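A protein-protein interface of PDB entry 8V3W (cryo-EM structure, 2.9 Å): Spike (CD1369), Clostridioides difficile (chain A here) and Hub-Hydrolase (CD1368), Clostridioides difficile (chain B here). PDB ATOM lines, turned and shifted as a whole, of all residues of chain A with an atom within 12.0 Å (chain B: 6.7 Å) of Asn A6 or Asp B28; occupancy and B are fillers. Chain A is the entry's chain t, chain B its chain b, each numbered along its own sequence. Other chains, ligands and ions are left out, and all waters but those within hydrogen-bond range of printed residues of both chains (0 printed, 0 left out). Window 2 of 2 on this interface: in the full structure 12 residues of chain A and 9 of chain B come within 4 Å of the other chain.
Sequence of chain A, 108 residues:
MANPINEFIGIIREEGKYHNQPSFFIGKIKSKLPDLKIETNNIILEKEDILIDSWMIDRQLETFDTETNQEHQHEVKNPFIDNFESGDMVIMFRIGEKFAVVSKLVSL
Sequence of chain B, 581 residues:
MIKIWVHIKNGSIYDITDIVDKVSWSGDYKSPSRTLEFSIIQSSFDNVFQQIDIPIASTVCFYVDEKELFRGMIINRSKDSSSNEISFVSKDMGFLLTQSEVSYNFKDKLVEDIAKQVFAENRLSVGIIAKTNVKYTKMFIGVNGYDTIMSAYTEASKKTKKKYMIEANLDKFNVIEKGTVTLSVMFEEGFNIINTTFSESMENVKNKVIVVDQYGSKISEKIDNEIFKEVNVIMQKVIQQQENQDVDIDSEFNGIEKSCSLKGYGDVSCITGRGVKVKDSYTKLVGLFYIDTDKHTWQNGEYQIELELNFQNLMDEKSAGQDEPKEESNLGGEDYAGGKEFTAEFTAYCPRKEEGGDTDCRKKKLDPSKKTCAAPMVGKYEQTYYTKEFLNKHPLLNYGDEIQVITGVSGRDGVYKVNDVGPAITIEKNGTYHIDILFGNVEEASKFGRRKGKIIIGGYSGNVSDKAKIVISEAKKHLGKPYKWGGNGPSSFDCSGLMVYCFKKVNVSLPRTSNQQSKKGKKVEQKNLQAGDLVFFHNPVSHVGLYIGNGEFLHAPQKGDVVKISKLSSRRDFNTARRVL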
ATOM      1  N   ALA A   2      26.578 -19.303   4.720  1.00  0.00           N
ATOM      2  CA  ALA A   2      26.796 -18.045   5.418  1.00  0.00           C
ATOM      3  C   ALA A   2      26.141 -16.881   4.686  1.00  0.00           C
ATOM      4  O   ALA A   2      26.523 -16.543   3.570  1.00  0.00           O
ATOM      5  CB  ALA A   2      28.278 -17.788   5.589  1.00  0.00           C
ATOM      6  N   ASN A   3      25.152 -16.280   5.323  1.00  0.00           N
ATOM      7  CA  ASN A   3      24.502 -15.090   4.790  1.00  0.00           C
ATOM      8  C   ASN A   3      25.425 -13.887   4.953  1.00  0.00           C
ATOM      9  O   ASN A   3      25.889 -13.619   6.064  1.00  0.00           O
ATOM     10  CB  ASN A   3      23.182 -14.852   5.512  1.00  0.00           C
ATOM     11  CG  ASN A   3      22.402 -13.697   4.940  1.00  0.00           C
ATOM     12  OD1 ASN A   3      22.462 -12.585   5.452  1.00  0.00           O
ATOM     13  ND2 ASN A   3      21.645 -13.959   3.887  1.00  0.00           N
ATOM     14  N   PRO A   4      25.724 -13.154   3.876  1.00  0.00           N
ATOM     15  CA  PRO A   4      26.698 -12.053   3.980  1.00  0.00           C
ATOM     16  C   PRO A   4      26.310 -10.952   4.954  1.00  0.00           C
ATOM     17  O   PRO A   4      27.202 -10.332   5.543  1.00  0.00           O
ATOM     18  CB  PRO A   4      26.782 -11.525   2.540  1.00  0.00           C
ATOM     19  CG  PRO A   4      25.596 -12.088   1.835  1.00  0.00           C
ATOM     20  CD  PRO A   4      25.291 -13.383   2.492  1.00  0.00           C
ATOM     21  N   ILE A   5      25.018 -10.675   5.136  1.00  0.00           N
ATOM     22  CA  ILE A   5      24.606  -9.612   6.051  1.00  0.00           C
ATOM     23  C   ILE A   5      24.983  -9.953   7.488  1.00  0.00           C
ATOM     24  O   ILE A   5      25.501  -9.105   8.229  1.00  0.00           O
ATOM     25  CB  ILE A   5      23.097  -9.347   5.912  1.00  0.00           C
ATOM     26  CG1 ILE A   5      22.767  -8.841   4.510  1.00  0.00           C
ATOM     27  CG2 ILE A   5      22.634  -8.353   6.951  1.00  0.00           C
ATOM     28  CD1 ILE A   5      23.273  -7.457   4.225  1.00  0.00           C
ATOM     29  N   ASN A   6      24.727 -11.192   7.909  1.00  0.00           N
ATOM     30  CA  ASN A   6      25.089 -11.609   9.258  1.00  0.00           C
ATOM     31  C   ASN A   6      26.597 -11.565   9.463  1.00  0.00           C
ATOM     32  O   ASN A   6      27.077 -11.187  10.538  1.00  0.00           O
ATOM     33  CB  ASN A   6      24.550 -13.010   9.530  1.00  0.00           C
ATOM     34  CG  ASN A   6      23.051 -13.100   9.362  1.00  0.00           C
ATOM     35  OD1 ASN A   6      22.394 -12.122   9.019  1.00  0.00           O
ATOM     36  ND2 ASN A   6      22.502 -14.279   9.602  1.00  0.00           N
ATOM     37  N   GLU A   7      27.362 -11.950   8.441  1.00  0.00           N
ATOM     38  CA  GLU A   7      28.814 -11.878   8.531  1.00  0.00           C
ATOM     39  C   GLU A   7      29.287 -10.438   8.667  1.00  0.00           C
ATOM     40  O   GLU A   7      30.213 -10.153   9.433  1.00  0.00           O
ATOM     41  CB  GLU A   7      29.444 -12.533   7.306  1.00  0.00           C
ATOM     42  CG  GLU A   7      29.081 -13.989   7.129  1.00  0.00           C
ATOM     43  CD  GLU A   7      29.766 -14.876   8.142  1.00  0.00           C
ATOM     44  OE1 GLU A   7      30.989 -14.723   8.327  1.00  0.00           O
ATOM     45  OE2 GLU A   7      29.089 -15.729   8.750  1.00  0.00           O
ATOM     46  N   PHE A   8      28.664  -9.519   7.930  1.00  0.00           N
ATOM     47  CA  PHE A   8      29.007  -8.106   8.052  1.00  0.00           C
ATOM     48  C   PHE A   8      28.716  -7.580   9.450  1.00  0.00           C
ATOM     49  O   PHE A   8      29.519  -6.832  10.022  1.00  0.00           O
ATOM     50  CB  PHE A   8      28.239  -7.299   7.007  1.00  0.00           C
ATOM     51  CG  PHE A   8      28.728  -5.894   6.845  1.00  0.00           C
ATOM     52  CD1 PHE A   8      30.007  -5.640   6.392  1.00  0.00           C
ATOM     53  CD2 PHE A   8      27.905  -4.827   7.141  1.00  0.00           C
ATOM     54  CE1 PHE A   8      30.457  -4.352   6.243  1.00  0.00           C
ATOM     55  CE2 PHE A   8      28.351  -3.536   6.994  1.00  0.00           C
ATOM     56  CZ  PHE A   8      29.629  -3.299   6.543  1.00  0.00           C
ATOM     57  N   ILE A   9      27.568  -7.955  10.016  1.00  0.00           N
ATOM     58  CA  ILE A   9      27.226  -7.499  11.363  1.00  0.00           C
ATOM     59  C   ILE A   9      28.218  -8.053  12.379  1.00  0.00           C
ATOM     60  O   ILE A   9      28.660  -7.340  13.291  1.00  0.00           O
ATOM     61  CB  ILE A   9      25.776  -7.885  11.709  1.00  0.00           C
ATOM     62  CG1 ILE A   9      24.800  -7.034  10.902  1.00  0.00           C
ATOM     63  CG2 ILE A   9      25.510  -7.696  13.184  1.00  0.00           C
ATOM     64  CD1 ILE A   9      23.391  -7.550  10.898  1.00  0.00           C
ATOM     65  N   GLY A  10      28.589  -9.326  12.237  1.00  0.00           N
ATOM     66  CA  GLY A  10      29.592  -9.895  13.124  1.00  0.00           C
ATOM     67  C   GLY A  10      30.939  -9.211  12.999  1.00  0.00           C
ATOM     68  O   GLY A  10      31.638  -9.004  13.995  1.00  0.00           O
ATOM     69  N   ILE A  11      31.318  -8.845  11.774  1.00  0.00           N
ATOM     70  CA  ILE A  11      32.572  -8.135  11.548  1.00  0.00           C
ATOM     71  C   ILE A  11      32.548  -6.776  12.234  1.00  0.00           C
ATOM     72  O   ILE A  11      33.537  -6.354  12.842  1.00  0.00           O
ATOM     73  CB  ILE A  11      32.840  -8.010  10.037  1.00  0.00           C
ATOM     74  CG1 ILE A  11      33.403  -9.321   9.492  1.00  0.00           C
ATOM     75  CG2 ILE A  11      33.781  -6.858   9.746  1.00  0.00           C
ATOM     76  CD1 ILE A  11      33.661  -9.302   8.011  1.00  0.00           C
ATOM     77  N   ILE A  12      31.425  -6.063  12.137  1.00  0.00           N
ATOM     78  CA  ILE A  12      31.305  -4.776  12.823  1.00  0.00           C
ATOM     79  C   ILE A  12      31.442  -4.962  14.328  1.00  0.00           C
ATOM     80  O   ILE A  12      32.169  -4.222  15.001  1.00  0.00           O
ATOM     81  CB  ILE A  12      29.976  -4.089  12.467  1.00  0.00           C
ATOM     82  CG1 ILE A  12      29.935  -3.718  10.988  1.00  0.00           C
ATOM     83  CG2 ILE A  12      29.773  -2.861  13.324  1.00  0.00           C
ATOM     84  CD1 ILE A  12      28.627  -3.107  10.563  1.00  0.00           C
ATOM     85  N   ARG A  13      30.744  -5.957  14.877  1.00  0.00           N
ATOM     86  CA  ARG A  13      30.802  -6.185  16.317  1.00  0.00           C
ATOM     87  C   ARG A  13      32.220  -6.504  16.770  1.00  0.00           C
ATOM     88  O   ARG A  13      32.644  -6.074  17.847  1.00  0.00           O
ATOM     89  CB  ARG A  13      29.852  -7.311  16.714  1.00  0.00           C
ATOM     90  CG  ARG A  13      28.388  -6.960  16.584  1.00  0.00           C
ATOM     91  CD  ARG A  13      27.532  -8.201  16.659  1.00  0.00           C
ATOM     92  NE  ARG A  13      26.124  -7.883  16.851  1.00  0.00           N
ATOM     93  CZ  ARG A  13      25.177  -8.787  17.050  1.00  0.00           C
ATOM     94  NH1 ARG A  13      25.453 -10.078  17.090  1.00  0.00           N
ATOM     95  NH2 ARG A  13      23.921  -8.384  17.210  1.00  0.00           N
ATOM     96  N   GLU A  14      32.965  -7.270  15.970  1.00  0.00           N
ATOM     97  CA  GLU A  14      34.325  -7.631  16.362  1.00  0.00           C
ATOM     98  C   GLU A  14      35.289  -6.459  16.223  1.00  0.00           C
ATOM     99  O   GLU A  14      36.097  -6.210  17.122  1.00  0.00           O
ATOM    100  CB  GLU A  14      34.813  -8.825  15.544  1.00  0.00           C
ATOM    101  CG  GLU A  14      34.085 -10.120  15.849  1.00  0.00           C
ATOM    102  CD  GLU A  14      34.444 -10.703  17.201  1.00  0.00           C
ATOM    103  OE1 GLU A  14      35.359 -10.173  17.866  1.00  0.00           O
ATOM    104  OE2 GLU A  14      33.802 -11.697  17.606  1.00  0.00           O
ATOM    105  N   GLU A  15      35.229  -5.727  15.109  1.00  0.00           N
ATOM    106  CA  GLU A  15      36.160  -4.622  14.904  1.00  0.00           C
ATOM    107  C   GLU A  15      35.849  -3.426  15.787  1.00  0.00           C
ATOM    108  O   GLU A  15      36.708  -2.555  15.947  1.00  0.00           O
ATOM    109  CB  GLU A  15      36.169  -4.176  13.442  1.00  0.00           C
ATOM    110  CG  GLU A  15      36.849  -5.140  12.490  1.00  0.00           C
ATOM    111  CD  GLU A  15      38.340  -5.246  12.735  1.00  0.00           C
ATOM    112  OE1 GLU A  15      38.931  -4.281  13.260  1.00  0.00           O
ATOM    113  OE2 GLU A  15      38.927  -6.295  12.400  1.00  0.00           O
ATOM    114  N   SER B  26      13.525 -18.429   2.910  1.00  0.00           N
ATOM    115  CA  SER B  26      14.945 -18.578   3.206  1.00  0.00           C
ATOM    116  C   SER B  26      15.188 -18.603   4.708  1.00  0.00           C
ATOM    117  O   SER B  26      14.330 -18.238   5.509  1.00  0.00           O
ATOM    118  CB  SER B  26      15.765 -17.458   2.561  1.00  0.00           C
ATOM    119  OG  SER B  26      15.428 -16.196   3.102  1.00  0.00           O
ATOM    120  N   GLY B  27      16.391 -19.037   5.072  1.00  0.00           N
ATOM    121  CA  GLY B  27      16.825 -19.045   6.456  1.00  0.00           C
ATOM    122  C   GLY B  27      18.321 -19.241   6.540  1.00  0.00           C
ATOM    123  O   GLY B  27      18.963 -19.676   5.579  1.00  0.00           O
ATOM    124  N   ASP B  28      18.873 -18.909   7.705  1.00  0.00           N
ATOM    125  CA  ASP B  28      20.306 -19.014   7.949  1.00  0.00           C
ATOM    126  C   ASP B  28      20.538 -19.623   9.322  1.00  0.00           C
ATOM    127  O   ASP B  28      19.675 -19.572  10.198  1.00  0.00           O
ATOM    128  CB  ASP B  28      21.004 -17.653   7.854  1.00  0.00           C
ATOM    129  CG  ASP B  28      22.509 -17.778   7.730  1.00  0.00           C
ATOM    130  OD1 ASP B  28      22.971 -18.617   6.933  1.00  0.00           O
ATOM    131  OD2 ASP B  28      23.232 -17.037   8.426  1.00  0.00           O
ATOM    132  N   TYR B  29      21.722 -20.201   9.506  1.00  0.00           N
ATOM    133  CA  TYR B  29      22.018 -20.905  10.746  1.00  0.00           C
ATOM    134  C   TYR B  29      22.435 -19.982  11.883  1.00  0.00           C
ATOM    135  O   TYR B  29      22.534 -20.444  13.023  1.00  0.00           O
ATOM    136  CB  TYR B  29      23.103 -21.962  10.511  1.00  0.00           C
ATOM    137  CG  TYR B  29      24.511 -21.425  10.411  1.00  0.00           C
ATOM    138  CD1 TYR B  29      24.857 -20.511   9.431  1.00  0.00           C
ATOM    139  CD2 TYR B  29      25.498 -21.848  11.285  1.00  0.00           C
ATOM    140  CE1 TYR B  29      26.139 -20.024   9.329  1.00  0.00           C
ATOM    141  CE2 TYR B  29      26.787 -21.366  11.193  1.00  0.00           C
ATOM    142  CZ  TYR B  29      27.102 -20.454  10.212  1.00  0.00           C
ATOM    143  OH  TYR B  29      28.383 -19.964  10.107  1.00  0.00           O
ATOM    144  N   LYS B  30      22.664 -18.701  11.613  1.00  0.00           N
ATOM    145  CA  LYS B  30      23.067 -17.752  12.640  1.00  0.00           C
ATOM    146  C   LYS B  30      21.914 -16.894  13.144  1.00  0.00           C
ATOM    147  O   LYS B  30      22.147 -15.961  13.913  1.00  0.00           O
ATOM    148  CB  LYS B  30      24.192 -16.861  12.122  1.00  0.00           C
ATOM    149  CG  LYS B  30      25.557 -17.335  12.558  1.00  0.00           C
ATOM    150  CD  LYS B  30      26.663 -16.544  11.911  1.00  0.00           C
ATOM    151  CE  LYS B  30      28.005 -17.094  12.337  1.00  0.00           C
ATOM    152  NZ  LYS B  30      27.959 -17.567  13.745  1.00  0.00           N
ATOM    153  N   SER B  31      20.687 -17.183  12.732  1.00  0.00           N
ATOM    154  CA  SER B  31      19.510 -16.490  13.221  1.00  0.00           C
ATOM    155  C   SER B  31      18.438 -17.501  13.590  1.00  0.00           C
ATOM    156  O   SER B  31      18.347 -18.565  12.975  1.00  0.00           O
ATOM    157  CB  SER B  31      18.965 -15.514  12.170  1.00  0.00           C
ATOM    158  OG  SER B  31      18.419 -16.209  11.069  1.00  0.00           O
ATOM    159  N   PRO B  32      17.618 -17.203  14.602  1.00  0.00           N
ATOM    160  CA  PRO B  32      16.588 -18.161  15.024  1.00  0.00           C
ATOM    161  C   PRO B  32      15.307 -18.116  14.209  1.00  0.00           C
ATOM    162  O   PRO B  32      14.437 -18.971  14.420  1.00  0.00           O
ATOM    163  CB  PRO B  32      16.315 -17.753  16.474  1.00  0.00           C
ATOM    164  CG  PRO B  32      16.601 -16.301  16.497  1.00  0.00           C
ATOM    165  CD  PRO B  32      17.741 -16.078  15.547  1.00  0.00           C
ATOM    166  N   SER B  33      15.149 -17.165  13.295  1.00  0.00           N
ATOM    167  CA  SER B  33      13.890 -16.979  12.593  1.00  0.00           C
ATOM    168  C   SER B  33      14.085 -17.096  11.088  1.00  0.00           C
ATOM    169  O   SER B  33      15.125 -16.722  10.547  1.00  0.00           O
ATOM    170  CB  SER B  33      13.268 -15.624  12.928  1.00  0.00           C
ATOM    171  OG  SER B  33      14.185 -14.577  12.694  1.00  0.00           O
ATOM    172  N   ARG B  34      13.070 -17.631  10.425  1.00  0.00           N
ATOM    173  CA  ARG B  34      13.018 -17.710   8.975  1.00  0.00           C
ATOM    174  C   ARG B  34      12.158 -16.580   8.429  1.00  0.00           C
ATOM    175  O   ARG B  34      11.354 -15.980   9.143  1.00  0.00           O
ATOM    176  CB  ARG B  34      12.466 -19.062   8.528  1.00  0.00           C
ATOM    177  CG  ARG B  34      13.395 -20.221   8.807  1.00  0.00           C
ATOM    178  CD  ARG B  34      12.965 -21.450   8.041  1.00  0.00           C
ATOM    179  NE  ARG B  34      14.072 -22.024   7.289  1.00  0.00           N
ATOM    180  CZ  ARG B  34      14.135 -22.071   5.967  1.00  0.00           C
ATOM    181  NH1 ARG B  34      13.159 -21.607   5.212  1.00  0.00           N
ATOM    182  NH2 ARG B  34      15.206 -22.598   5.389  1.00  0.00           N
ATOM    183  N   MET B 165      21.070 -26.091  17.134  1.00  0.00           N
ATOM    184  CA  MET B 165      20.407 -24.922  16.578  1.00  0.00           C
ATOM    185  C   MET B 165      19.006 -24.815  17.158  1.00  0.00           C
ATOM    186  O   MET B 165      18.454 -25.785  17.682  1.00  0.00           O
ATOM    187  CB  MET B 165      20.353 -24.988  15.050  1.00  0.00           C
ATOM    188  CG  MET B 165      19.379 -26.021  14.514  1.00  0.00           C
ATOM    189  SD  MET B 165      19.333 -26.092  12.714  1.00  0.00           S
ATOM    190  CE  MET B 165      19.860 -24.437  12.292  1.00  0.00           C
ATOM    191  N   THR B 272      18.107 -25.333   6.170  1.00  0.00           N
ATOM    192  CA  THR B 272      19.253 -25.180   7.056  1.00  0.00           C
ATOM    193  C   THR B 272      19.176 -26.157   8.223  1.00  0.00           C
ATOM    194  O   THR B 272      18.138 -26.288   8.874  1.00  0.00           O
ATOM    195  CB  THR B 272      19.314 -23.740   7.565  1.00  0.00           C
ATOM    196  OG1 THR B 272      19.742 -22.882   6.504  1.00  0.00           O
ATOM    197  CG2 THR B 272      20.280 -23.610   8.715  1.00  0.00           C
ATOM    198  N   ASP B 292      24.099 -24.670   5.561  1.00  0.00           N
ATOM    199  CA  ASP B 292      24.220 -23.496   6.413  1.00  0.00           C
ATOM    200  C   ASP B 292      23.267 -22.375   6.042  1.00  0.00           C
ATOM    201  O   ASP B 292      22.839 -21.632   6.922  1.00  0.00           O
ATOM    202  CB  ASP B 292      25.652 -22.952   6.364  1.00  0.00           C
ATOM    203  CG  ASP B 292      26.620 -23.782   7.173  1.00  0.00           C
ATOM    204  OD1 ASP B 292      26.165 -24.634   7.962  1.00  0.00           O
ATOM    205  OD2 ASP B 292      27.842 -23.588   7.014  1.00  0.00           O
ATOM    206  N   THR B 293      22.941 -22.231   4.762  1.00  0.00           N
ATOM    207  CA  THR B 293      22.035 -21.202   4.282  1.00  0.00           C
ATOM    208  C   THR B 293      21.278 -21.762   3.091  1.00  0.00           C
ATOM    209  O   THR B 293      21.824 -22.540   2.309  1.00  0.00           O
ATOM    210  CB  THR B 293      22.787 -19.926   3.887  1.00  0.00           C
ATOM    211  OG1 THR B 293      23.688 -19.558   4.938  1.00  0.00           O
ATOM    212  CG2 THR B 293      21.827 -18.779   3.626  1.00  0.00           C
ATOM    213  N   ASP B 294      20.017 -21.364   2.959  1.00  0.00           N
ATOM    214  CA  ASP B 294      19.195 -21.849   1.863  1.00  0.00           C
ATOM    215  C   ASP B 294      18.249 -20.748   1.417  1.00  0.00           C
ATOM    216  O   ASP B 294      17.973 -19.803   2.156  1.00  0.00           O
ATOM    217  CB  ASP B 294      18.416 -23.102   2.263  1.00  0.00           C
ATOM    218  CG  ASP B 294      17.301 -22.805   3.230  1.00  0.00           C
ATOM    219  OD1 ASP B 294      16.234 -22.342   2.787  1.00  0.00           O
ATOM    220  OD2 ASP B 294      17.483 -23.034   4.440  1.00  0.00           O
ATOM    221  N   GLU B 308      24.236 -23.006   0.683  1.00  0.00           N
ATOM    222  CA  GLU B 308      25.605 -22.810   1.147  1.00  0.00           C
ATOM    223  C   GLU B 308      25.985 -24.025   1.980  1.00  0.00           C
ATOM    224  O   GLU B 308      25.410 -24.258   3.046  1.00  0.00           O
ATOM    225  CB  GLU B 308      25.739 -21.522   1.952  1.00  0.00           C
ATOM    226  CG  GLU B 308      25.355 -20.275   1.190  1.00  0.00           C
ATOM    227  CD  GLU B 308      26.400 -19.859   0.175  1.00  0.00           C
ATOM    228  OE1 GLU B 308      27.604 -20.034   0.445  1.00  0.00           O
ATOM    229  OE2 GLU B 308      26.016 -19.348  -0.896  1.00  0.00           O
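Ala A2 touches Glu B308 (N to CB, 3.6 Å).
OD1 of Asp B28 touches N of Asn A3 (3.6 Å).
OG1 of Thr B293 touches N of Asn A3, 3.6 Å away.
Asn A6 touches Lys B30.
OE2 of Glu A7 touches CE of Lys B30, 3.99 Å away.
Pro A4 touches none of the printed residues of chain B.
Printed residues of chain B within 4 Å of Asn A6: Asp B28 and Lys B30.
Printed residues of chain B within 4 Å of Glu A7: Lys B30.
Ile A12 touches none of the printed residues of chain B.
No residue of chain A comes within 4 Å of Ser B26.
Of the printed residues of chain A, Asp B28 touches Asn A3 (3.6 Å) and Asn A6 (3.1 Å).
No residue of chain A comes within 4 Å of Ser B31.
No residue of chain A comes within 4 Å of Pro B32.
No residue of chain A comes within 4 Å of Thr B272.
No residue of chain A comes within 4 Å of Asp B292.
Of chain A, only Ala A2 (2.9 Å) and Asn A3 (3.6 Å) come within 4 Å of Thr B293.
Printed residues of chain A within 4 Å of Glu B308: Ala A2.
The nearest printed residue of chain B that does not touch Asn A6 is Ser B31 (4.5 Å).
Of the 15 printed residues of chain B, 4 touch a printed residue of chain A.
Of the 14 printed residues of chain A, 4 touch a printed residue of chain B.
The backbone carbonyl oxygen (O) of Glu B308 sits at hydrogen-bond distance from the backbone NH (N) of Asp B292.
The backbone carbonyl oxygen of Thr B293 lies within hydrogen-bond range of the backbone NH of Glu B308 (2.9 Å).
The side-chain amide oxygen of Asn A3 is in hydrogen-bond range of the backbone NH of Ile A5 (3.2 Å).
N of Ala A2 lies within hydrogen-bond range of OG1 of Thr B293, at 2.9 Å.
ND2 of Asn A6 lies within hydrogen-bond range of OD2 of Asp B28.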
